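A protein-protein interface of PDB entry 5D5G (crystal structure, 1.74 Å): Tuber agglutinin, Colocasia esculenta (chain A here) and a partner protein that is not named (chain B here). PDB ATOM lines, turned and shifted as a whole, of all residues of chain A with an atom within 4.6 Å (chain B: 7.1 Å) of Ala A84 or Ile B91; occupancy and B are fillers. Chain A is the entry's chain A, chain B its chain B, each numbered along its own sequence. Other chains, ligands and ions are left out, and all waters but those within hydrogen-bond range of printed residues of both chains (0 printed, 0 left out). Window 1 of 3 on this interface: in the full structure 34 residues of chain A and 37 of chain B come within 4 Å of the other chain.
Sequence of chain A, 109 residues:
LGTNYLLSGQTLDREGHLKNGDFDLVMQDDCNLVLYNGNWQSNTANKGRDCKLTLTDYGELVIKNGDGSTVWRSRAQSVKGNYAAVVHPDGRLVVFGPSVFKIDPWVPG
Of the printed residues of chain B, Tyr A5 touches Asn B7, Ile B91, Arg B93 and Asp B94.
Printed residues of chain B within 4 Å of Ala A84: Ile B91 and Tyr B101.
Of the printed residues of chain B, Val A94 touches Trp B106 (3.1 Å).
Printed residues of chain B within 4 Å of Val A95: Trp B106 (2.6 Å).
Of the printed residues of chain A, Ile B91 touches Tyr A5, Ala A84 and Val A86.
The nearest residue of chain B that does not touch Ala A84 is Val B89 (5.8 Å).
The nearest printed residue of chain A that does not touch Ile B91 is Leu A7 (5.0 Å).
The nearest printed residue of chain B that does not touch Tyr A5 is Leu B92 (4.6 Å).
The backbone NH (N) of Val B89 sits at hydrogen-bond distance from the backbone carbonyl oxygen (O) of Tyr B101, 2.9 Å away.
The side-chain hydroxyl (OH) of Tyr B101 lies within hydrogen-bond range of the guanidinium group (NH1) of Arg B93.
N of Leu B92 sits at hydrogen-bond distance from O of Asn B7 (2.8 Å).
O of Val B99 sits close to N of Ile B91 (2.8 Å).
O of Val A86 is in hydrogen-bond range of N of Val A94, 3.0 Å away.
The backbone carbonyl oxygen (O) of Ala A84 lies within hydrogen-bond range of the backbone NH (N) of Phe A96, 2.5 Å away.
Of the 19 printed residues of chain B, 7 touch a printed residue of chain A.
Hydrophobic or aromatic side chains of chain B within 4 Å of the printed part of chain A: Val B89, Ile B91 and Tyr B101.
Of the 11 printed residues of chain A, 8 touch a printed residue of chain B.
Printed residues of chain A that touch a printed residue of chain B: Tyr A5, Leu A7, Tyr A83, Ala A84, Val A86, Val A94, Val A95 and Phe A96.
Among the printed residues, 14 pairs touch across the chains.
CE2 of Tyr A5 touches ND2 of Asn B7, at 3.8 Å.
Ile B91 touches Tyr A5.
Tyr A5 touches Arg B93 (OH to CA, 3.2 Å).
Arg B93 touches Leu A7.
OH of Tyr B101 touches CD2 of Leu A7, 3.8 Å away.
Tyr B101 touches Tyr A83.
CB of Ala A84 touches CD1 of Ile B91, 3.9 Å away.
CB of Ala A84 touches CD2 of Tyr B101, 3.8 Å away.
Val A94 touches Trp B106.
CG1 of Val B89 touches CD2 of Phe A96, 3.7 Å away.
O of Trp B106 lies within hydrogen-bond range of N of Val A95 (2.6 Å).
N of Asp B94 sits at hydrogen-bond distance from OH of Tyr A5 (2.6 Å).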
ATOM      1  N   TYR A   5     -11.285  12.097  -0.876  1.00  0.00           N
ATOM      2  CA  TYR A   5     -10.060  12.802  -0.485  1.00  0.00           C
ATOM      3  C   TYR A   5      -8.803  12.264  -1.139  1.00  0.00           C
ATOM      4  O   TYR A   5      -8.762  11.142  -1.628  1.00  0.00           O
ATOM      5  CB  TYR A   5      -9.863  12.850   1.038  1.00  0.00           C
ATOM      6  CG  TYR A   5      -9.593  11.529   1.748  1.00  0.00           C
ATOM      7  CD1 TYR A   5      -8.319  10.978   1.790  1.00  0.00           C
ATOM      8  CD2 TYR A   5     -10.600  10.884   2.459  1.00  0.00           C
ATOM      9  CE1 TYR A   5      -8.060   9.783   2.464  1.00  0.00           C
ATOM     10  CE2 TYR A   5     -10.354   9.695   3.136  1.00  0.00           C
ATOM     11  CZ  TYR A   5      -9.089   9.150   3.136  1.00  0.00           C
ATOM     12  OH  TYR A   5      -8.862   7.964   3.816  1.00  0.00           O
ATOM     13  N   LEU A   6      -7.768  13.088  -1.114  1.00  0.00           N
ATOM     14  CA  LEU A   6      -6.448  12.697  -1.557  1.00  0.00           C
ATOM     15  C   LEU A   6      -5.434  13.218  -0.533  1.00  0.00           C
ATOM     16  O   LEU A   6      -5.286  14.426  -0.366  1.00  0.00           O
ATOM     17  CB  LEU A   6      -6.174  13.305  -2.929  1.00  0.00           C
ATOM     18  CG  LEU A   6      -4.713  13.229  -3.377  1.00  0.00           C
ATOM     19  CD1 LEU A   6      -4.305  11.788  -3.620  1.00  0.00           C
ATOM     20  CD2 LEU A   6      -4.495  14.069  -4.614  1.00  0.00           C
ATOM     21  N   LEU A   7      -4.750  12.319   0.170  1.00  0.00           N
ATOM     22  CA  LEU A   7      -3.779  12.748   1.176  1.00  0.00           C
ATOM     23  C   LEU A   7      -2.425  13.054   0.517  1.00  0.00           C
ATOM     24  O   LEU A   7      -2.044  12.393  -0.454  1.00  0.00           O
ATOM     25  CB  LEU A   7      -3.623  11.692   2.280  1.00  0.00           C
ATOM     26  CG  LEU A   7      -4.871  11.363   3.103  1.00  0.00           C
ATOM     27  CD1 LEU A   7      -4.581  10.348   4.216  1.00  0.00           C
ATOM     28  CD2 LEU A   7      -5.465  12.637   3.657  1.00  0.00           C
ATOM     29  N   LEU A  55      -0.165  15.216  -4.204  1.00  0.00           N
ATOM     30  CA  LEU A  55      -0.274  16.321  -3.254  1.00  0.00           C
ATOM     31  C   LEU A  55       1.037  16.505  -2.508  1.00  0.00           C
ATOM     32  O   LEU A  55       1.532  15.575  -1.867  1.00  0.00           O
ATOM     33  CB  LEU A  55      -1.427  16.080  -2.270  1.00  0.00           C
ATOM     34  CG  LEU A  55      -1.789  17.194  -1.284  1.00  0.00           C
ATOM     35  CD1 LEU A  55      -2.127  18.470  -2.036  1.00  0.00           C
ATOM     36  CD2 LEU A  55      -2.971  16.759  -0.401  1.00  0.00           C
ATOM     37  N   TYR A  83      -1.462  17.162   4.184  1.00  0.00           N
ATOM     38  CA  TYR A  83      -2.521  17.982   3.615  1.00  0.00           C
ATOM     39  C   TYR A  83      -3.647  17.119   3.053  1.00  0.00           C
ATOM     40  O   TYR A  83      -3.550  15.884   3.022  1.00  0.00           O
ATOM     41  CB  TYR A  83      -1.967  18.887   2.521  1.00  0.00           C
ATOM     42  CG  TYR A  83      -1.138  20.048   3.018  1.00  0.00           C
ATOM     43  CD1 TYR A  83       0.063  19.842   3.680  1.00  0.00           C
ATOM     44  CD2 TYR A  83      -1.546  21.354   2.801  1.00  0.00           C
ATOM     45  CE1 TYR A  83       0.832  20.907   4.134  1.00  0.00           C
ATOM     46  CE2 TYR A  83      -0.788  22.422   3.244  1.00  0.00           C
ATOM     47  CZ  TYR A  83       0.393  22.193   3.911  1.00  0.00           C
ATOM     48  OH  TYR A  83       1.135  23.266   4.349  1.00  0.00           O
ATOM     49  N   ALA A  84      -4.704  17.785   2.599  1.00  0.00           N
ATOM     50  CA  ALA A  84      -5.851  17.099   2.029  1.00  0.00           C
ATOM     51  C   ALA A  84      -6.561  17.957   0.986  1.00  0.00           C
ATOM     52  O   ALA A  84      -6.937  19.108   1.244  1.00  0.00           O
ATOM     53  CB  ALA A  84      -6.815  16.682   3.123  1.00  0.00           C
ATOM     54  N   ALA A  85      -6.700  17.394  -0.209  1.00  0.00           N
ATOM     55  CA  ALA A  85      -7.559  17.949  -1.237  1.00  0.00           C
ATOM     56  C   ALA A  85      -8.847  17.174  -1.082  1.00  0.00           C
ATOM     57  O   ALA A  85      -8.823  15.945  -0.993  1.00  0.00           O
ATOM     58  CB  ALA A  85      -6.969  17.693  -2.603  1.00  0.00           C
ATOM     59  N   VAL A  86      -9.978  17.861  -1.024  1.00  0.00           N
ATOM     60  CA  VAL A  86     -11.226  17.141  -0.865  1.00  0.00           C
ATOM     61  C   VAL A  86     -12.326  17.745  -1.726  1.00  0.00           C
ATOM     62  O   VAL A  86     -12.389  18.967  -1.895  1.00  0.00           O
ATOM     63  CB  VAL A  86     -11.642  17.125   0.582  1.00  0.00           C
ATOM     64  CG1 VAL A  86     -10.725  16.218   1.377  1.00  0.00           C
ATOM     65  CG2 VAL A  86     -11.582  18.514   1.129  1.00  0.00           C
ATOM     66  N   VAL A  94     -11.149  21.588  -2.808  1.00  0.00           N
ATOM     67  CA  VAL A  94     -10.484  22.536  -1.890  1.00  0.00           C
ATOM     68  C   VAL A  94      -9.322  21.897  -1.133  1.00  0.00           C
ATOM     69  O   VAL A  94      -9.500  20.880  -0.468  1.00  0.00           O
ATOM     70  CB  VAL A  94     -11.469  23.095  -0.849  1.00  0.00           C
ATOM     71  CG1 VAL A  94     -10.769  24.109   0.045  1.00  0.00           C
ATOM     72  CG2 VAL A  94     -12.669  23.732  -1.529  1.00  0.00           C
ATOM     73  N   VAL A  95      -8.130  22.485  -1.229  1.00  0.00           N
ATOM     74  CA  VAL A  95      -6.982  21.944  -0.510  1.00  0.00           C
ATOM     75  C   VAL A  95      -7.068  22.386   0.945  1.00  0.00           C
ATOM     76  O   VAL A  95      -7.342  23.551   1.204  1.00  0.00           O
ATOM     77  CB  VAL A  95      -5.661  22.435  -1.114  1.00  0.00           C
ATOM     78  CG1 VAL A  95      -4.480  21.847  -0.359  1.00  0.00           C
ATOM     79  CG2 VAL A  95      -5.588  22.067  -2.587  1.00  0.00           C
ATOM     80  N   PHE A  96      -6.848  21.471   1.887  1.00  0.00           N
ATOM     81  CA  PHE A  96      -6.963  21.801   3.311  1.00  0.00           C
ATOM     82  C   PHE A  96      -5.700  21.495   4.093  1.00  0.00           C
ATOM     83  O   PHE A  96      -5.211  20.366   4.059  1.00  0.00           O
ATOM     84  CB  PHE A  96      -8.118  21.025   3.971  1.00  0.00           C
ATOM     85  CG  PHE A  96      -9.461  21.624   3.728  1.00  0.00           C
ATOM     86  CD1 PHE A  96      -9.898  22.695   4.480  1.00  0.00           C
ATOM     87  CD2 PHE A  96     -10.283  21.127   2.727  1.00  0.00           C
ATOM     88  CE1 PHE A  96     -11.128  23.262   4.241  1.00  0.00           C
ATOM     89  CE2 PHE A  96     -11.522  21.684   2.478  1.00  0.00           C
ATOM     90  CZ  PHE A  96     -11.945  22.755   3.239  1.00  0.00           C
ATOM     91  N   ASN B   7     -17.881  10.861   5.567  1.00  0.00           N
ATOM     92  CA  ASN B   7     -16.655  10.836   6.386  1.00  0.00           C
ATOM     93  C   ASN B   7     -15.991  12.191   6.669  1.00  0.00           C
ATOM     94  O   ASN B   7     -14.862  12.259   7.175  1.00  0.00           O
ATOM     95  CB  ASN B   7     -15.632   9.848   5.811  1.00  0.00           C
ATOM     96  CG  ASN B   7     -15.132  10.263   4.462  1.00  0.00           C
ATOM     97  OD1 ASN B   7     -15.724  11.130   3.812  1.00  0.00           O
ATOM     98  ND2 ASN B   7     -14.030   9.645   4.019  1.00  0.00           N
ATOM     99  N   LEU B   8     -16.710  13.257   6.348  1.00  0.00           N
ATOM    100  CA  LEU B   8     -16.220  14.607   6.518  1.00  0.00           C
ATOM    101  C   LEU B   8     -17.035  15.278   7.603  1.00  0.00           C
ATOM    102  O   LEU B   8     -18.212  14.976   7.795  1.00  0.00           O
ATOM    103  CB  LEU B   8     -16.381  15.381   5.209  1.00  0.00           C
ATOM    104  CG  LEU B   8     -15.854  14.643   3.964  1.00  0.00           C
ATOM    105  CD1 LEU B   8     -15.990  15.487   2.704  1.00  0.00           C
ATOM    106  CD2 LEU B   8     -14.408  14.178   4.144  1.00  0.00           C
ATOM    107  N   LEU B   9     -16.406  16.174   8.342  1.00  0.00           N
ATOM    108  CA  LEU B   9     -17.165  17.116   9.127  1.00  0.00           C
ATOM    109  C   LEU B   9     -16.513  18.457   8.930  1.00  0.00           C
ATOM    110  O   LEU B   9     -15.451  18.731   9.488  1.00  0.00           O
ATOM    111  CB  LEU B   9     -17.195  16.747  10.603  1.00  0.00           C
ATOM    112  CG  LEU B   9     -18.171  17.635  11.394  1.00  0.00           C
ATOM    113  CD1 LEU B   9     -19.592  17.246  11.088  1.00  0.00           C
ATOM    114  CD2 LEU B   9     -17.924  17.578  12.884  1.00  0.00           C
ATOM    115  N   LEU B  21     -19.673   9.731  12.080  1.00  0.00           N
ATOM    116  CA  LEU B  21     -18.935   9.655  10.829  1.00  0.00           C
ATOM    117  C   LEU B  21     -18.672   8.185  10.553  1.00  0.00           C
ATOM    118  O   LEU B  21     -18.530   7.385  11.481  1.00  0.00           O
ATOM    119  CB  LEU B  21     -17.604  10.414  10.913  1.00  0.00           C
ATOM    120  CG  LEU B  21     -17.549  11.942  11.001  1.00  0.00           C
ATOM    121  CD1 LEU B  21     -16.110  12.416  10.870  1.00  0.00           C
ATOM    122  CD2 LEU B  21     -18.391  12.616   9.946  1.00  0.00           C
ATOM    123  N   ALA B  23     -16.469   5.387   7.864  1.00  0.00           N
ATOM    124  CA  ALA B  23     -15.518   5.172   6.792  1.00  0.00           C
ATOM    125  C   ALA B  23     -15.126   3.718   6.880  1.00  0.00           C
ATOM    126  O   ALA B  23     -14.434   3.312   7.818  1.00  0.00           O
ATOM    127  CB  ALA B  23     -14.312   6.082   6.916  1.00  0.00           C
ATOM    128  N   LEU B  28     -16.929   7.421  14.042  1.00  0.00           N
ATOM    129  CA  LEU B  28     -16.601   8.361  15.089  1.00  0.00           C
ATOM    130  C   LEU B  28     -17.937   8.922  15.505  1.00  0.00           C
ATOM    131  O   LEU B  28     -18.646   9.493  14.678  1.00  0.00           O
ATOM    132  CB  LEU B  28     -15.722   9.471  14.531  1.00  0.00           C
ATOM    133  CG  LEU B  28     -15.340  10.560  15.519  1.00  0.00           C
ATOM    134  CD1 LEU B  28     -14.749   9.947  16.770  1.00  0.00           C
ATOM    135  CD2 LEU B  28     -14.358  11.511  14.870  1.00  0.00           C
ATOM    136  N   VAL B  89     -11.717  21.085   7.855  1.00  0.00           N
ATOM    137  CA  VAL B  89     -12.507  19.863   7.760  1.00  0.00           C
ATOM    138  C   VAL B  89     -11.842  18.782   8.579  1.00  0.00           C
ATOM    139  O   VAL B  89     -10.615  18.666   8.592  1.00  0.00           O
ATOM    140  CB  VAL B  89     -12.769  19.400   6.266  1.00  0.00           C
ATOM    141  CG1 VAL B  89     -11.481  19.024   5.535  1.00  0.00           C
ATOM    142  CG2 VAL B  89     -13.746  18.234   6.200  1.00  0.00           C
ATOM    143  N   LEU B  90     -12.663  18.034   9.308  1.00  0.00           N
ATOM    144  CA  LEU B  90     -12.244  16.801   9.954  1.00  0.00           C
ATOM    145  C   LEU B  90     -12.567  15.647   9.008  1.00  0.00           C
ATOM    146  O   LEU B  90     -13.667  15.577   8.479  1.00  0.00           O
ATOM    147  CB  LEU B  90     -13.019  16.613  11.256  1.00  0.00           C
ATOM    148  CG  LEU B  90     -13.176  15.212  11.847  1.00  0.00           C
ATOM    149  CD1 LEU B  90     -11.839  14.538  12.156  1.00  0.00           C
ATOM    150  CD2 LEU B  90     -14.039  15.272  13.098  1.00  0.00           C
ATOM    151  N   ILE B  91     -11.616  14.746   8.802  1.00  0.00           N
ATOM    152  CA  ILE B  91     -11.835  13.600   7.940  1.00  0.00           C
ATOM    153  C   ILE B  91     -11.791  12.369   8.818  1.00  0.00           C
ATOM    154  O   ILE B  91     -11.055  12.361   9.782  1.00  0.00           O
ATOM    155  CB  ILE B  91     -10.740  13.520   6.865  1.00  0.00           C
ATOM    156  CG1 ILE B  91     -10.964  14.604   5.814  1.00  0.00           C
ATOM    157  CG2 ILE B  91     -10.713  12.156   6.209  1.00  0.00           C
ATOM    158  CD1 ILE B  91      -9.758  14.879   4.975  1.00  0.00           C
ATOM    159  N   LEU B  92     -12.615  11.363   8.528  1.00  0.00           N
ATOM    160  CA  LEU B  92     -12.395  10.029   9.071  1.00  0.00           C
ATOM    161  C   LEU B  92     -11.752   9.187   7.973  1.00  0.00           C
ATOM    162  O   LEU B  92     -12.441   8.628   7.105  1.00  0.00           O
ATOM    163  CB  LEU B  92     -13.706   9.402   9.574  1.00  0.00           C
ATOM    164  CG  LEU B  92     -13.664   7.934  10.031  1.00  0.00           C
ATOM    165  CD1 LEU B  92     -12.635   7.678  11.118  1.00  0.00           C
ATOM    166  CD2 LEU B  92     -15.032   7.475  10.501  1.00  0.00           C
ATOM    167  N   ARG B  93     -10.422   9.120   7.998  1.00  0.00           N
ATOM    168  CA  ARG B  93      -9.655   8.497   6.918  1.00  0.00           C
ATOM    169  C   ARG B  93      -9.722   6.967   6.934  1.00  0.00           C
ATOM    170  O   ARG B  93      -9.894   6.360   7.996  1.00  0.00           O
ATOM    171  CB  ARG B  93      -8.202   8.952   6.997  1.00  0.00           C
ATOM    172  CG  ARG B  93      -8.012  10.278   7.689  1.00  0.00           C
ATOM    173  CD  ARG B  93      -6.582  10.754   7.526  1.00  0.00           C
ATOM    174  NE  ARG B  93      -5.619   9.657   7.621  1.00  0.00           N
ATOM    175  CZ  ARG B  93      -4.317   9.835   7.832  1.00  0.00           C
ATOM    176  NH1 ARG B  93      -3.830  11.071   7.977  1.00  0.00           N
ATOM    177  NH2 ARG B  93      -3.505   8.784   7.907  1.00  0.00           N
ATOM    178  N   ASP B  94      -9.566   6.349   5.761  1.00  0.00           N
ATOM    179  CA  ASP B  94      -9.651   4.889   5.647  1.00  0.00           C
ATOM    180  C   ASP B  94      -8.742   4.150   6.636  1.00  0.00           C
ATOM    181  O   ASP B  94      -9.043   3.010   7.007  1.00  0.00           O
ATOM    182  CB  ASP B  94      -9.338   4.404   4.220  1.00  0.00           C
ATOM    183  CG  ASP B  94     -10.166   5.104   3.153  1.00  0.00           C
ATOM    184  OD1 ASP B  94     -11.338   5.439   3.411  1.00  0.00           O
ATOM    185  OD2 ASP B  94      -9.633   5.323   2.043  1.00  0.00           O
ATOM    186  N   GLY B  96      -8.403   4.915   9.637  1.00  0.00           N
ATOM    187  CA  GLY B  96      -9.051   4.947  10.933  1.00  0.00           C
ATOM    188  C   GLY B  96      -8.640   6.157  11.747  1.00  0.00           C
ATOM    189  O   GLY B  96      -9.167   6.411  12.827  1.00  0.00           O
ATOM    190  N   PHE B  97      -7.685   6.911  11.234  1.00  0.00           N
ATOM    191  CA  PHE B  97      -7.314   8.149  11.876  1.00  0.00           C
ATOM    192  C   PHE B  97      -8.431   9.123  11.633  1.00  0.00           C
ATOM    193  O   PHE B  97      -9.090   9.075  10.596  1.00  0.00           O
ATOM    194  CB  PHE B  97      -6.029   8.699  11.272  1.00  0.00           C
ATOM    195  CG  PHE B  97      -4.801   8.020  11.768  1.00  0.00           C
ATOM    196  CD1 PHE B  97      -4.720   6.646  11.801  1.00  0.00           C
ATOM    197  CD2 PHE B  97      -3.729   8.753  12.207  1.00  0.00           C
ATOM    198  CE1 PHE B  97      -3.596   6.019  12.258  1.00  0.00           C
ATOM    199  CE2 PHE B  97      -2.600   8.122  12.669  1.00  0.00           C
ATOM    200  CZ  PHE B  97      -2.540   6.747  12.691  1.00  0.00           C
ATOM    201  N   ALA B  98      -8.651   9.996  12.605  1.00  0.00           N
ATOM    202  CA  ALA B  98      -9.566  11.104  12.442  1.00  0.00           C
ATOM    203  C   ALA B  98      -8.709  12.335  12.557  1.00  0.00           C
ATOM    204  O   ALA B  98      -8.218  12.621  13.643  1.00  0.00           O
ATOM    205  N   VAL B  99      -8.504  13.049  11.455  1.00  0.00           N
ATOM    206  CA  VAL B  99      -7.620  14.194  11.463  1.00  0.00           C
ATOM    207  C   VAL B  99      -8.355  15.454  11.022  1.00  0.00           C
ATOM    208  O   VAL B  99      -9.241  15.396  10.174  1.00  0.00           O
ATOM    209  CB  VAL B  99      -6.397  13.937  10.553  1.00  0.00           C
ATOM    210  CG1 VAL B  99      -5.343  15.019  10.728  1.00  0.00           C
ATOM    211  CG2 VAL B  99      -5.803  12.563  10.842  1.00  0.00           C
ATOM    212  N   ILE B 100      -8.006  16.590  11.629  1.00  0.00           N
ATOM    213  CA  ILE B 100      -8.482  17.897  11.193  1.00  0.00           C
ATOM    214  C   ILE B 100      -7.484  18.500  10.191  1.00  0.00           C
ATOM    215  O   ILE B 100      -6.276  18.299  10.330  1.00  0.00           O
ATOM    216  CB  ILE B 100      -8.642  18.835  12.392  1.00  0.00           C
ATOM    217  CG1 ILE B 100      -9.530  18.168  13.448  1.00  0.00           C
ATOM    218  CG2 ILE B 100      -9.253  20.150  11.958  1.00  0.00           C
ATOM    219  CD1 ILE B 100      -9.924  19.067  14.621  1.00  0.00           C
ATOM    220  N   TYR B 101      -7.992  19.220   9.188  1.00  0.00           N
ATOM    221  CA  TYR B 101      -7.173  19.869   8.163  1.00  0.00           C
ATOM    222  C   TYR B 101      -7.668  21.290   7.943  1.00  0.00           C
ATOM    223  O   TYR B 101      -8.880  21.530   7.912  1.00  0.00           O
ATOM    224  CB  TYR B 101      -7.217  19.095   6.826  1.00  0.00           C
ATOM    225  CG  TYR B 101      -6.589  17.723   6.904  1.00  0.00           C
ATOM    226  CD1 TYR B 101      -7.317  16.639   7.349  1.00  0.00           C
ATOM    227  CD2 TYR B 101      -5.262  17.511   6.545  1.00  0.00           C
ATOM    228  CE1 TYR B 101      -6.755  15.370   7.435  1.00  0.00           C
ATOM    229  CE2 TYR B 101      -4.687  16.236   6.630  1.00  0.00           C
ATOM    230  CZ  TYR B 101      -5.446  15.169   7.078  1.00  0.00           C
ATOM    231  OH  TYR B 101      -4.906  13.888   7.180  1.00  0.00           O
ATOM    232  N   TRP B 106      -6.660  26.785  -0.951  1.00  0.00           N
ATOM    233  CA  TRP B 106      -6.923  26.739  -2.385  1.00  0.00           C
ATOM    234  C   TRP B 106      -8.224  26.016  -2.660  1.00  0.00           C
ATOM    235  O   TRP B 106      -8.418  24.880  -2.210  1.00  0.00           O
ATOM    236  CB  TRP B 106      -5.778  26.060  -3.136  1.00  0.00           C
ATOM    237  CG  TRP B 106      -5.813  26.300  -4.616  1.00  0.00           C
ATOM    238  CD1 TRP B 106      -5.247  27.343  -5.296  1.00  0.00           C
ATOM    239  CD2 TRP B 106      -6.444  25.477  -5.599  1.00  0.00           C
ATOM    240  NE1 TRP B 106      -5.492  27.215  -6.643  1.00  0.00           N
ATOM    241  CE2 TRP B 106      -6.230  26.080  -6.852  1.00  0.00           C
ATOM    242  CE3 TRP B 106      -7.178  24.289  -5.539  1.00  0.00           C
ATOM    243  CZ2 TRP B 106      -6.720  25.536  -8.030  1.00  0.00           C
ATOM    244  CZ3 TRP B 106      -7.667  23.752  -6.708  1.00  0.00           C
ATOM    245  CH2 TRP B 106      -7.436  24.373  -7.938  1.00  0.00           C
